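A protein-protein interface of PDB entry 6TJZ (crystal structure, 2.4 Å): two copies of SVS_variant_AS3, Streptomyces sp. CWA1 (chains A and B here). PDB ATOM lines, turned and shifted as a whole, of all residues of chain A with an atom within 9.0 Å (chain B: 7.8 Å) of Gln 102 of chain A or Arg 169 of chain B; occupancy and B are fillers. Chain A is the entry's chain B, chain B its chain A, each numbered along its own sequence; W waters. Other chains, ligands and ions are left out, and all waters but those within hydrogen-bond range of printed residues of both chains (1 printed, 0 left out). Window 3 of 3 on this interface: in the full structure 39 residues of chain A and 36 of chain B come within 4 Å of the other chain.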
ATOM      1  N   PHE A  86     -26.541 -14.451 -13.662  1.00  0.00           N
ATOM      2  CA  PHE A  86     -26.897 -13.238 -14.448  1.00  0.00           C
ATOM      3  C   PHE A  86     -27.960 -12.430 -13.704  1.00  0.00           C
ATOM      4  O   PHE A  86     -27.775 -11.197 -13.650  1.00  0.00           O
ATOM      5  CB  PHE A  86     -27.387 -13.586 -15.857  1.00  0.00           C
ATOM      6  CG  PHE A  86     -27.703 -12.399 -16.735  1.00  0.00           C
ATOM      7  CD1 PHE A  86     -26.693 -11.586 -17.224  1.00  0.00           C
ATOM      8  CD2 PHE A  86     -29.009 -12.111 -17.104  1.00  0.00           C
ATOM      9  CE1 PHE A  86     -26.979 -10.509 -18.045  1.00  0.00           C
ATOM     10  CE2 PHE A  86     -29.299 -11.036 -17.931  1.00  0.00           C
ATOM     11  CZ  PHE A  86     -28.280 -10.235 -18.397  1.00  0.00           C
ATOM     12  N   THR A  98     -29.292  -2.654 -11.332  1.00  0.00           N
ATOM     13  CA  THR A  98     -29.171  -2.248 -12.763  1.00  0.00           C
ATOM     14  C   THR A  98     -30.449  -1.513 -13.195  1.00  0.00           C
ATOM     15  O   THR A  98     -31.554  -2.098 -13.036  1.00  0.00           O
ATOM     16  CB  THR A  98     -28.895  -3.450 -13.682  1.00  0.00           C
ATOM     17  OG1 THR A  98     -27.781  -4.177 -13.176  1.00  0.00           O
ATOM     18  CG2 THR A  98     -28.573  -3.060 -15.107  1.00  0.00           C
ATOM     19  N   ARG A  99     -30.295  -0.290 -13.722  1.00  0.00           N
ATOM     20  CA  ARG A  99     -31.398   0.592 -14.199  1.00  0.00           C
ATOM     21  C   ARG A  99     -31.877   0.122 -15.577  1.00  0.00           C
ATOM     22  O   ARG A  99     -31.086  -0.352 -16.391  1.00  0.00           O
ATOM     23  CB  ARG A  99     -30.918   2.049 -14.247  1.00  0.00           C
ATOM     24  CG  ARG A  99     -30.494   2.630 -12.903  1.00  0.00           C
ATOM     25  CD  ARG A  99     -31.642   2.788 -11.914  1.00  0.00           C
ATOM     26  NE  ARG A  99     -32.717   3.561 -12.525  1.00  0.00           N
ATOM     27  CZ  ARG A  99     -33.962   3.664 -12.066  1.00  0.00           C
ATOM     28  NH1 ARG A  99     -34.324   3.058 -10.944  1.00  0.00           N
ATOM     29  NH2 ARG A  99     -34.842   4.389 -12.743  1.00  0.00           N
ATOM     30  N   PRO A 100     -33.178   0.278 -15.904  1.00  0.00           N
ATOM     31  CA  PRO A 100     -33.727  -0.151 -17.190  1.00  0.00           C
ATOM     32  C   PRO A 100     -32.940   0.257 -18.444  1.00  0.00           C
ATOM     33  O   PRO A 100     -32.767  -0.572 -19.326  1.00  0.00           O
ATOM     34  CB  PRO A 100     -35.074   0.566 -17.235  1.00  0.00           C
ATOM     35  CG  PRO A 100     -35.483   0.646 -15.791  1.00  0.00           C
ATOM     36  CD  PRO A 100     -34.197   0.876 -15.033  1.00  0.00           C
ATOM     37  N   ALA A 101     -32.541   1.528 -18.511  1.00  0.00           N
ATOM     38  CA  ALA A 101     -31.729   2.103 -19.610  1.00  0.00           C
ATOM     39  C   ALA A 101     -30.428   1.309 -19.811  1.00  0.00           C
ATOM     40  O   ALA A 101     -30.135   0.926 -20.934  1.00  0.00           O
ATOM     41  CB  ALA A 101     -31.485   3.569 -19.339  1.00  0.00           C
ATOM     42  N   GLN A 102     -29.646   1.030 -18.777  1.00  0.00           N
ATOM     43  CA  GLN A 102     -28.373   0.275 -18.960  1.00  0.00           C
ATOM     44  C   GLN A 102     -28.725  -1.184 -19.302  1.00  0.00           C
ATOM     45  O   GLN A 102     -28.077  -1.774 -20.193  1.00  0.00           O
ATOM     46  CB  GLN A 102     -27.474   0.411 -17.724  1.00  0.00           C
ATOM     47  CG  GLN A 102     -26.834   1.782 -17.542  1.00  0.00           C
ATOM     48  CD  GLN A 102     -27.782   2.888 -17.113  1.00  0.00           C
ATOM     49  OE1 GLN A 102     -28.973   2.690 -16.878  1.00  0.00           O
ATOM     50  NE2 GLN A 102     -27.266   4.101 -17.039  1.00  0.00           N
ATOM     51  N   PHE A 103     -29.779  -1.723 -18.679  1.00  0.00           N
ATOM     52  CA  PHE A 103     -30.214  -3.130 -18.834  1.00  0.00           C
ATOM     53  C   PHE A 103     -30.546  -3.436 -20.292  1.00  0.00           C
ATOM     54  O   PHE A 103     -30.097  -4.483 -20.808  1.00  0.00           O
ATOM     55  CB  PHE A 103     -31.434  -3.468 -17.986  1.00  0.00           C
ATOM     56  CG  PHE A 103     -31.669  -4.947 -18.011  1.00  0.00           C
ATOM     57  CD1 PHE A 103     -30.802  -5.784 -17.356  1.00  0.00           C
ATOM     58  CD2 PHE A 103     -32.622  -5.497 -18.842  1.00  0.00           C
ATOM     59  CE1 PHE A 103     -30.937  -7.159 -17.456  1.00  0.00           C
ATOM     60  CE2 PHE A 103     -32.755  -6.867 -18.947  1.00  0.00           C
ATOM     61  CZ  PHE A 103     -31.917  -7.694 -18.244  1.00  0.00           C
ATOM     62  N   ASN A 104     -31.332  -2.562 -20.915  1.00  0.00           N
ATOM     63  CA  ASN A 104     -31.797  -2.729 -22.310  1.00  0.00           C
ATOM     64  C   ASN A 104     -30.552  -2.897 -23.189  1.00  0.00           C
ATOM     65  O   ASN A 104     -30.513  -3.829 -23.994  1.00  0.00           O
ATOM     66  CB  ASN A 104     -32.701  -1.573 -22.733  1.00  0.00           C
ATOM     67  CG  ASN A 104     -34.074  -1.576 -22.084  1.00  0.00           C
ATOM     68  OD1 ASN A 104     -34.395  -2.441 -21.263  1.00  0.00           O
ATOM     69  ND2 ASN A 104     -34.906  -0.611 -22.474  1.00  0.00           N
ATOM     70  N   ALA A 105     -29.538  -2.064 -23.009  1.00  0.00           N
ATOM     71  CA  ALA A 105     -28.225  -2.191 -23.699  1.00  0.00           C
ATOM     72  C   ALA A 105     -27.576  -3.537 -23.336  1.00  0.00           C
ATOM     73  O   ALA A 105     -27.156  -4.263 -24.259  1.00  0.00           O
ATOM     74  CB  ALA A 105     -27.293  -1.049 -23.345  1.00  0.00           C
ATOM     75  N   LEU A 106     -27.471  -3.844 -22.046  1.00  0.00           N
ATOM     76  CA  LEU A 106     -26.786  -5.080 -21.577  1.00  0.00           C
ATOM     77  C   LEU A 106     -27.494  -6.317 -22.143  1.00  0.00           C
ATOM     78  O   LEU A 106     -26.794  -7.238 -22.543  1.00  0.00           O
ATOM     79  CB  LEU A 106     -26.762  -5.151 -20.051  1.00  0.00           C
ATOM     80  CG  LEU A 106     -26.174  -6.449 -19.501  1.00  0.00           C
ATOM     81  CD1 LEU A 106     -24.741  -6.647 -19.983  1.00  0.00           C
ATOM     82  CD2 LEU A 106     -26.243  -6.490 -17.979  1.00  0.00           C
ATOM     83  N   ALA A 107     -28.829  -6.318 -22.162  1.00  0.00           N
ATOM     84  CA  ALA A 107     -29.659  -7.411 -22.699  1.00  0.00           C
ATOM     85  C   ALA A 107     -29.313  -7.579 -24.175  1.00  0.00           C
ATOM     86  O   ALA A 107     -29.150  -8.714 -24.607  1.00  0.00           O
ATOM     87  CB  ALA A 107     -31.136  -7.106 -22.508  1.00  0.00           C
ATOM     88  N   GLY A 108     -29.265  -6.471 -24.912  1.00  0.00           N
ATOM     89  CA  GLY A 108     -28.897  -6.421 -26.337  1.00  0.00           C
ATOM     90  C   GLY A 108     -27.507  -6.998 -26.589  1.00  0.00           C
ATOM     91  O   GLY A 108     -27.376  -7.837 -27.496  1.00  0.00           O
ATOM     92  N   ARG A 109     -26.515  -6.598 -25.791  1.00  0.00           N
ATOM     93  CA  ARG A 109     -25.107  -7.049 -25.930  1.00  0.00           C
ATOM     94  C   ARG A 109     -25.035  -8.546 -25.643  1.00  0.00           C
ATOM     95  O   ARG A 109     -24.504  -9.293 -26.458  1.00  0.00           O
ATOM     96  CB  ARG A 109     -24.176  -6.289 -24.982  1.00  0.00           C
ATOM     97  CG  ARG A 109     -23.210  -5.341 -25.680  1.00  0.00           C
ATOM     98  CD  ARG A 109     -22.363  -4.571 -24.682  1.00  0.00           C
ATOM     99  NE  ARG A 109     -23.028  -3.320 -24.428  1.00  0.00           N
ATOM    100  CZ  ARG A 109     -23.420  -2.868 -23.244  1.00  0.00           C
ATOM    101  NH1 ARG A 109     -23.178  -3.538 -22.124  1.00  0.00           N
ATOM    102  NH2 ARG A 109     -24.046  -1.703 -23.199  1.00  0.00           N
ATOM    103  N   VAL A 110     -25.592  -8.983 -24.529  1.00  0.00           N
ATOM    104  CA  VAL A 110     -25.446 -10.398 -24.110  1.00  0.00           C
ATOM    105  C   VAL A 110     -26.075 -11.291 -25.187  1.00  0.00           C
ATOM    106  O   VAL A 110     -25.415 -12.266 -25.602  1.00  0.00           O
ATOM    107  CB  VAL A 110     -26.029 -10.577 -22.705  1.00  0.00           C
ATOM    108  CG1 VAL A 110     -26.163 -12.032 -22.322  1.00  0.00           C
ATOM    109  CG2 VAL A 110     -25.152  -9.857 -21.702  1.00  0.00           C
ATOM    110  N   ASP A 124     -17.049  -7.676 -19.890  1.00  0.00           N
ATOM    111  CA  ASP A 124     -18.341  -8.132 -19.303  1.00  0.00           C
ATOM    112  C   ASP A 124     -18.201  -9.614 -18.899  1.00  0.00           C
ATOM    113  O   ASP A 124     -17.724 -10.426 -19.724  1.00  0.00           O
ATOM    114  CB  ASP A 124     -19.496  -7.854 -20.264  1.00  0.00           C
ATOM    115  CG  ASP A 124     -20.850  -8.151 -19.654  1.00  0.00           C
ATOM    116  OD1 ASP A 124     -21.089  -9.322 -19.332  1.00  0.00           O
ATOM    117  OD2 ASP A 124     -21.636  -7.206 -19.491  1.00  0.00           O
ATOM    118  N   ALA A 161     -36.305  -7.245 -18.566  1.00  0.00           N
ATOM    119  CA  ALA A 161     -36.366  -5.805 -18.904  1.00  0.00           C
ATOM    120  C   ALA A 161     -37.708  -5.235 -18.463  1.00  0.00           C
ATOM    121  O   ALA A 161     -37.747  -4.098 -17.974  1.00  0.00           O
ATOM    122  CB  ALA A 161     -36.152  -5.592 -20.379  1.00  0.00           C
ATOM    123  N   ILE A 164     -37.776  -5.122 -14.486  1.00  0.00           N
ATOM    124  CA  ILE A 164     -36.873  -4.038 -13.995  1.00  0.00           C
ATOM    125  C   ILE A 164     -37.541  -2.693 -14.300  1.00  0.00           C
ATOM    126  O   ILE A 164     -37.499  -1.779 -13.435  1.00  0.00           O
ATOM    127  CB  ILE A 164     -35.480  -4.183 -14.625  1.00  0.00           C
ATOM    128  CG1 ILE A 164     -34.726  -5.326 -13.948  1.00  0.00           C
ATOM    129  CG2 ILE A 164     -34.701  -2.875 -14.598  1.00  0.00           C
ATOM    130  CD1 ILE A 164     -33.621  -5.895 -14.801  1.00  0.00           C
ATOM    131  N   THR B  98     -37.766   8.370 -24.409  1.00  0.00           N
ATOM    132  CA  THR B  98     -36.714   8.677 -23.403  1.00  0.00           C
ATOM    133  C   THR B  98     -37.065   8.018 -22.066  1.00  0.00           C
ATOM    134  O   THR B  98     -36.439   8.416 -21.054  1.00  0.00           O
ATOM    135  CB  THR B  98     -36.558  10.196 -23.208  1.00  0.00           C
ATOM    136  OG1 THR B  98     -37.854  10.784 -23.060  1.00  0.00           O
ATOM    137  CG2 THR B  98     -35.829  10.863 -24.355  1.00  0.00           C
ATOM    138  N   PRO B 100     -37.358   4.275 -21.036  1.00  0.00           N
ATOM    139  CA  PRO B 100     -37.203   2.851 -21.291  1.00  0.00           C
ATOM    140  C   PRO B 100     -38.042   1.994 -20.344  1.00  0.00           C
ATOM    141  O   PRO B 100     -38.566   0.995 -20.816  1.00  0.00           O
ATOM    142  CB  PRO B 100     -35.715   2.556 -21.089  1.00  0.00           C
ATOM    143  CG  PRO B 100     -35.120   3.828 -20.498  1.00  0.00           C
ATOM    144  CD  PRO B 100     -36.089   4.961 -20.753  1.00  0.00           C
ATOM    145  N   ALA B 161     -35.763  -0.874 -27.551  1.00  0.00           N
ATOM    146  CA  ALA B 161     -35.558  -0.790 -26.085  1.00  0.00           C
ATOM    147  C   ALA B 161     -34.125  -0.358 -25.815  1.00  0.00           C
ATOM    148  O   ALA B 161     -33.911   0.526 -24.975  1.00  0.00           O
ATOM    149  CB  ALA B 161     -35.838  -2.123 -25.422  1.00  0.00           C
ATOM    150  N   TRP B 162     -33.181  -0.975 -26.513  1.00  0.00           N
ATOM    151  CA  TRP B 162     -31.740  -0.605 -26.478  1.00  0.00           C
ATOM    152  C   TRP B 162     -31.574   0.858 -26.928  1.00  0.00           C
ATOM    153  O   TRP B 162     -30.980   1.640 -26.168  1.00  0.00           O
ATOM    154  CB  TRP B 162     -30.989  -1.581 -27.370  1.00  0.00           C
ATOM    155  CG  TRP B 162     -29.501  -1.553 -27.290  1.00  0.00           C
ATOM    156  CD1 TRP B 162     -28.666  -0.619 -26.741  1.00  0.00           C
ATOM    157  CD2 TRP B 162     -28.659  -2.542 -27.890  1.00  0.00           C
ATOM    158  NE1 TRP B 162     -27.359  -0.995 -26.904  1.00  0.00           N
ATOM    159  CE2 TRP B 162     -27.325  -2.160 -27.627  1.00  0.00           C
ATOM    160  CE3 TRP B 162     -28.917  -3.712 -28.611  1.00  0.00           C
ATOM    161  CZ2 TRP B 162     -26.253  -2.931 -28.062  1.00  0.00           C
ATOM    162  CZ3 TRP B 162     -27.852  -4.464 -29.044  1.00  0.00           C
ATOM    163  CH2 TRP B 162     -26.543  -4.088 -28.759  1.00  0.00           C
ATOM    164  N   GLN B 163     -32.123   1.226 -28.096  1.00  0.00           N
ATOM    165  CA  GLN B 163     -32.076   2.609 -28.642  1.00  0.00           C
ATOM    166  C   GLN B 163     -32.586   3.605 -27.585  1.00  0.00           C
ATOM    167  O   GLN B 163     -31.861   4.569 -27.277  1.00  0.00           O
ATOM    168  CB  GLN B 163     -32.871   2.692 -29.945  1.00  0.00           C
ATOM    169  CG  GLN B 163     -32.763   4.027 -30.671  1.00  0.00           C
ATOM    170  CD  GLN B 163     -33.147   3.865 -32.126  1.00  0.00           C
ATOM    171  OE1 GLN B 163     -32.331   3.466 -32.968  1.00  0.00           O
ATOM    172  NE2 GLN B 163     -34.411   4.134 -32.430  1.00  0.00           N
ATOM    173  N   ILE B 164     -33.775   3.370 -27.035  1.00  0.00           N
ATOM    174  CA  ILE B 164     -34.456   4.277 -26.069  1.00  0.00           C
ATOM    175  C   ILE B 164     -33.668   4.343 -24.758  1.00  0.00           C
ATOM    176  O   ILE B 164     -33.594   5.430 -24.167  1.00  0.00           O
ATOM    177  CB  ILE B 164     -35.900   3.830 -25.842  1.00  0.00           C
ATOM    178  CG1 ILE B 164     -36.733   4.111 -27.088  1.00  0.00           C
ATOM    179  CG2 ILE B 164     -36.483   4.490 -24.597  1.00  0.00           C
ATOM    180  CD1 ILE B 164     -38.059   3.416 -27.070  1.00  0.00           C
ATOM    181  N   GLY B 165     -33.119   3.225 -24.305  1.00  0.00           N
ATOM    182  CA  GLY B 165     -32.165   3.222 -23.183  1.00  0.00           C
ATOM    183  C   GLY B 165     -31.047   4.218 -23.447  1.00  0.00           C
ATOM    184  O   GLY B 165     -30.809   5.082 -22.572  1.00  0.00           O
ATOM    185  N   ASN B 166     -30.402   4.110 -24.615  1.00  0.00           N
ATOM    186  CA  ASN B 166     -29.267   4.984 -25.014  1.00  0.00           C
ATOM    187  C   ASN B 166     -29.736   6.453 -25.023  1.00  0.00           C
ATOM    188  O   ASN B 166     -28.993   7.311 -24.483  1.00  0.00           O
ATOM    189  CB  ASN B 166     -28.681   4.529 -26.351  1.00  0.00           C
ATOM    190  CG  ASN B 166     -27.955   3.201 -26.266  1.00  0.00           C
ATOM    191  OD1 ASN B 166     -27.767   2.649 -25.191  1.00  0.00           O
ATOM    192  ND2 ASN B 166     -27.523   2.679 -27.399  1.00  0.00           N
ATOM    193  N   GLN B 167     -30.931   6.744 -25.560  1.00  0.00           N
ATOM    194  CA  GLN B 167     -31.434   8.142 -25.699  1.00  0.00           C
ATOM    195  C   GLN B 167     -31.579   8.752 -24.303  1.00  0.00           C
ATOM    196  O   GLN B 167     -31.097   9.861 -24.120  1.00  0.00           O
ATOM    197  CB  GLN B 167     -32.761   8.257 -26.459  1.00  0.00           C
ATOM    198  CG  GLN B 167     -32.653   8.167 -27.982  1.00  0.00           C
ATOM    199  CD  GLN B 167     -31.772   9.204 -28.642  1.00  0.00           C
ATOM    200  OE1 GLN B 167     -31.121   8.933 -29.651  1.00  0.00           O
ATOM    201  NE2 GLN B 167     -31.744  10.406 -28.088  1.00  0.00           N
ATOM    202  N   ALA B 168     -32.197   8.040 -23.357  1.00  0.00           N
ATOM    203  CA  ALA B 168     -32.430   8.526 -21.978  1.00  0.00           C
ATOM    204  C   ALA B 168     -31.093   8.909 -21.330  1.00  0.00           C
ATOM    205  O   ALA B 168     -31.035   9.974 -20.720  1.00  0.00           O
ATOM    206  CB  ALA B 168     -33.154   7.485 -21.158  1.00  0.00           C
ATOM    207  N   ARG B 169     -30.058   8.076 -21.480  1.00  0.00           N
ATOM    208  CA  ARG B 169     -28.729   8.265 -20.838  1.00  0.00           C
ATOM    209  C   ARG B 169     -27.856   9.283 -21.584  1.00  0.00           C
ATOM    210  O   ARG B 169     -26.776   9.615 -21.048  1.00  0.00           O
ATOM    211  CB  ARG B 169     -27.957   6.948 -20.802  1.00  0.00           C
ATOM    212  CG  ARG B 169     -28.503   5.940 -19.807  1.00  0.00           C
ATOM    213  CD  ARG B 169     -28.071   4.561 -20.244  1.00  0.00           C
ATOM    214  NE  ARG B 169     -26.620   4.440 -20.290  1.00  0.00           N
ATOM    215  CZ  ARG B 169     -25.955   3.542 -21.008  1.00  0.00           C
ATOM    216  NH1 ARG B 169     -26.597   2.688 -21.801  1.00  0.00           N
ATOM    217  NH2 ARG B 169     -24.637   3.527 -20.946  1.00  0.00           N
ATOM    218  N   GLY B 170     -28.260   9.711 -22.781  1.00  0.00           N
ATOM    219  CA  GLY B 170     -27.428  10.524 -23.689  1.00  0.00           C
ATOM    220  C   GLY B 170     -26.181   9.758 -24.102  1.00  0.00           C
ATOM    221  O   GLY B 170     -25.145  10.406 -24.319  1.00  0.00           O
ATOM    222  N   HIS B 171     -26.282   8.424 -24.191  1.00  0.00           N
ATOM    223  CA  HIS B 171     -25.182   7.514 -24.600  1.00  0.00           C
ATOM    224  C   HIS B 171     -25.220   7.343 -26.114  1.00  0.00           C
ATOM    225  O   HIS B 171     -26.285   7.004 -26.650  1.00  0.00           O
ATOM    226  CB  HIS B 171     -25.273   6.167 -23.893  1.00  0.00           C
ATOM    227  CG  HIS B 171     -24.214   5.198 -24.284  1.00  0.00           C
ATOM    228  ND1 HIS B 171     -22.907   5.333 -23.872  1.00  0.00           N
ATOM    229  CD2 HIS B 171     -24.267   4.059 -25.003  1.00  0.00           C
ATOM    230  CE1 HIS B 171     -22.192   4.319 -24.325  1.00  0.00           C
ATOM    231  NE2 HIS B 171     -23.000   3.530 -25.031  1.00  0.00           N
ATOM    232  N   MET B 172     -24.098   7.665 -26.748  1.00  0.00           N
ATOM    233  CA  MET B 172     -23.799   7.460 -28.179  1.00  0.00           C
ATOM    234  C   MET B 172     -23.039   6.140 -28.277  1.00  0.00           C
ATOM    235  O   MET B 172     -21.917   6.040 -27.790  1.00  0.00           O
ATOM    236  CB  MET B 172     -22.961   8.628 -28.726  1.00  0.00           C
ATOM    237  CG  MET B 172     -22.757   8.611 -30.242  1.00  0.00           C
ATOM    238  SD  MET B 172     -24.305   8.468 -31.183  1.00  0.00           S
ATOM    239  CE  MET B 172     -25.126   9.966 -30.633  1.00  0.00           C
ATOM    240  N   ASP B 177     -21.667  -1.742 -30.898  1.00  0.00           N
ATOM    241  CA  ASP B 177     -23.014  -1.693 -30.267  1.00  0.00           C
ATOM    242  C   ASP B 177     -23.995  -1.094 -31.274  1.00  0.00           C
ATOM    243  O   ASP B 177     -25.139  -1.588 -31.340  1.00  0.00           O
ATOM    244  CB  ASP B 177     -23.050  -0.902 -28.949  1.00  0.00           C
ATOM    245  CG  ASP B 177     -22.442  -1.640 -27.762  1.00  0.00           C
ATOM    246  OD1 ASP B 177     -22.098  -2.814 -27.929  1.00  0.00           O
ATOM    247  OD2 ASP B 177     -22.313  -1.030 -26.681  1.00  0.00           O
ATOM    248  N   GLN B 244     -29.084   8.846 -32.664  1.00  0.00           N
ATOM    249  CA  GLN B 244     -28.159   7.697 -32.821  1.00  0.00           C
ATOM    250  C   GLN B 244     -28.256   7.204 -34.258  1.00  0.00           C
ATOM    251  O   GLN B 244     -29.296   6.660 -34.593  1.00  0.00           O
ATOM    252  CB  GLN B 244     -28.546   6.543 -31.903  1.00  0.00           C
ATOM    253  CG  GLN B 244     -28.257   6.822 -30.444  1.00  0.00           C
ATOM    254  CD  GLN B 244     -28.906   5.776 -29.578  1.00  0.00           C
ATOM    255  OE1 GLN B 244     -28.437   4.643 -29.471  1.00  0.00           O
ATOM    256  NE2 GLN B 244     -29.984   6.165 -28.932  1.00  0.00           N
HETATM  257  O   HOH W   1     -24.184   0.936 -23.021  1.00  0.00           O
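The side-chain amide nitrogen (ND2) of Asn 104 of chain A sits at hydrogen-bond distance from the backbone carbonyl oxygen (O) of Ala 161 of chain B, 2.9 Å away. The side-chain amide nitrogen (NE2) of Gln 102 of chain A lies close to the guanidinium group (NE) of Arg 169 of chain B, 3.3 Å away. The side-chain carboxylate (OD2) of Asp 177 of chain B is in salt-bridge range of the guanidinium group (NE) of Arg 109 of chain A (3.3 Å).
The side-chain amide oxygen (OD1) of Asn 104 of chain A lies close to the backbone carbonyl oxygen (O) of Pro 100 of chain A, at 3.1 Å.
Among the printed residues, merely in contact across the chains: Ala 105 of chain A with Trp 162 of chain B (3.5 Å), Gly 108 of chain A with Trp 162 of chain B (3.5 Å), Asn 104 of chain A with Pro 100 of chain B (3.6 Å), Ala 101 of chain A with Gly 165 of chain B (3.6 Å), Ala 101 of chain A with Arg 169 of chain B (3.7 Å), Ala 101 of chain A with Pro 100 of chain B (3.8 Å), Asn 104 of chain A with Trp 162 of chain B (3.9 Å) and Arg 109 of chain A with Trp 162 of chain B (3.9 Å).
Of chain B, only Arg 169 comes within 4 Å of Gln 102 of chain A. Printed residues of chain B within 4 Å of Asn 104 of chain A: Pro 100 (3.6 Å), Ala 161 (2.9 Å) and Trp 162 (3.9 Å). Of the printed residues of chain B, Ala 105 of chain A touches Trp 162. Leu 106 of chain A touches none of the printed residues of chain B. Of the printed residues of chain B, Gly 108 of chain A touches Trp 162 (3.5 Å). Of the printed residues of chain B, Arg 109 of chain A touches Trp 162 (3.9 Å) and Asp 177 (3.3 Å). Of the printed residues of chain A, Ala 161 of chain B touches Asn 104. Gln 167 of chain B touches none of the printed residues of chain A. Ala 168 of chain B touches none of the printed residues of chain A. Of chain A, only Ala 101 and Gln 102 come within 4 Å of Arg 169 of chain B. No residue of chain A comes within 4 Å of Gly 170 of chain B. The nearest residue of chain B that does not touch Gln 102 of chain A is Gly 165 of chain B (5.5 Å). The nearest residue of chain A that does not touch Arg 169 of chain B is Ala 105 of chain A (4.1 Å). The nearest printed residue of chain A that does not touch Pro 100 of chain B is Pro 100 of chain A (4.4 Å).
Of the 16 printed residues of chain B, 6 touch a printed residue of chain A. Printed residues of chain B that touch a printed residue of chain A: Pro 100, Ala 161, Trp 162, Gly 165, Arg 169 and Asp 177. Hydrophobic or aromatic side chains of chain A within 4 Å of the printed part of chain B: Ala 101 and Ala 105.
Positions printed for both chains: 98, 100, 161 and 164.
Water W1 lies within hydrogen-bond range of NH2 of Arg 109 of chain A (2.6 Å), NH1 of Arg 169 of chain B (3.2 Å) and NE2 of His 171 of chain B (3.5 Å).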
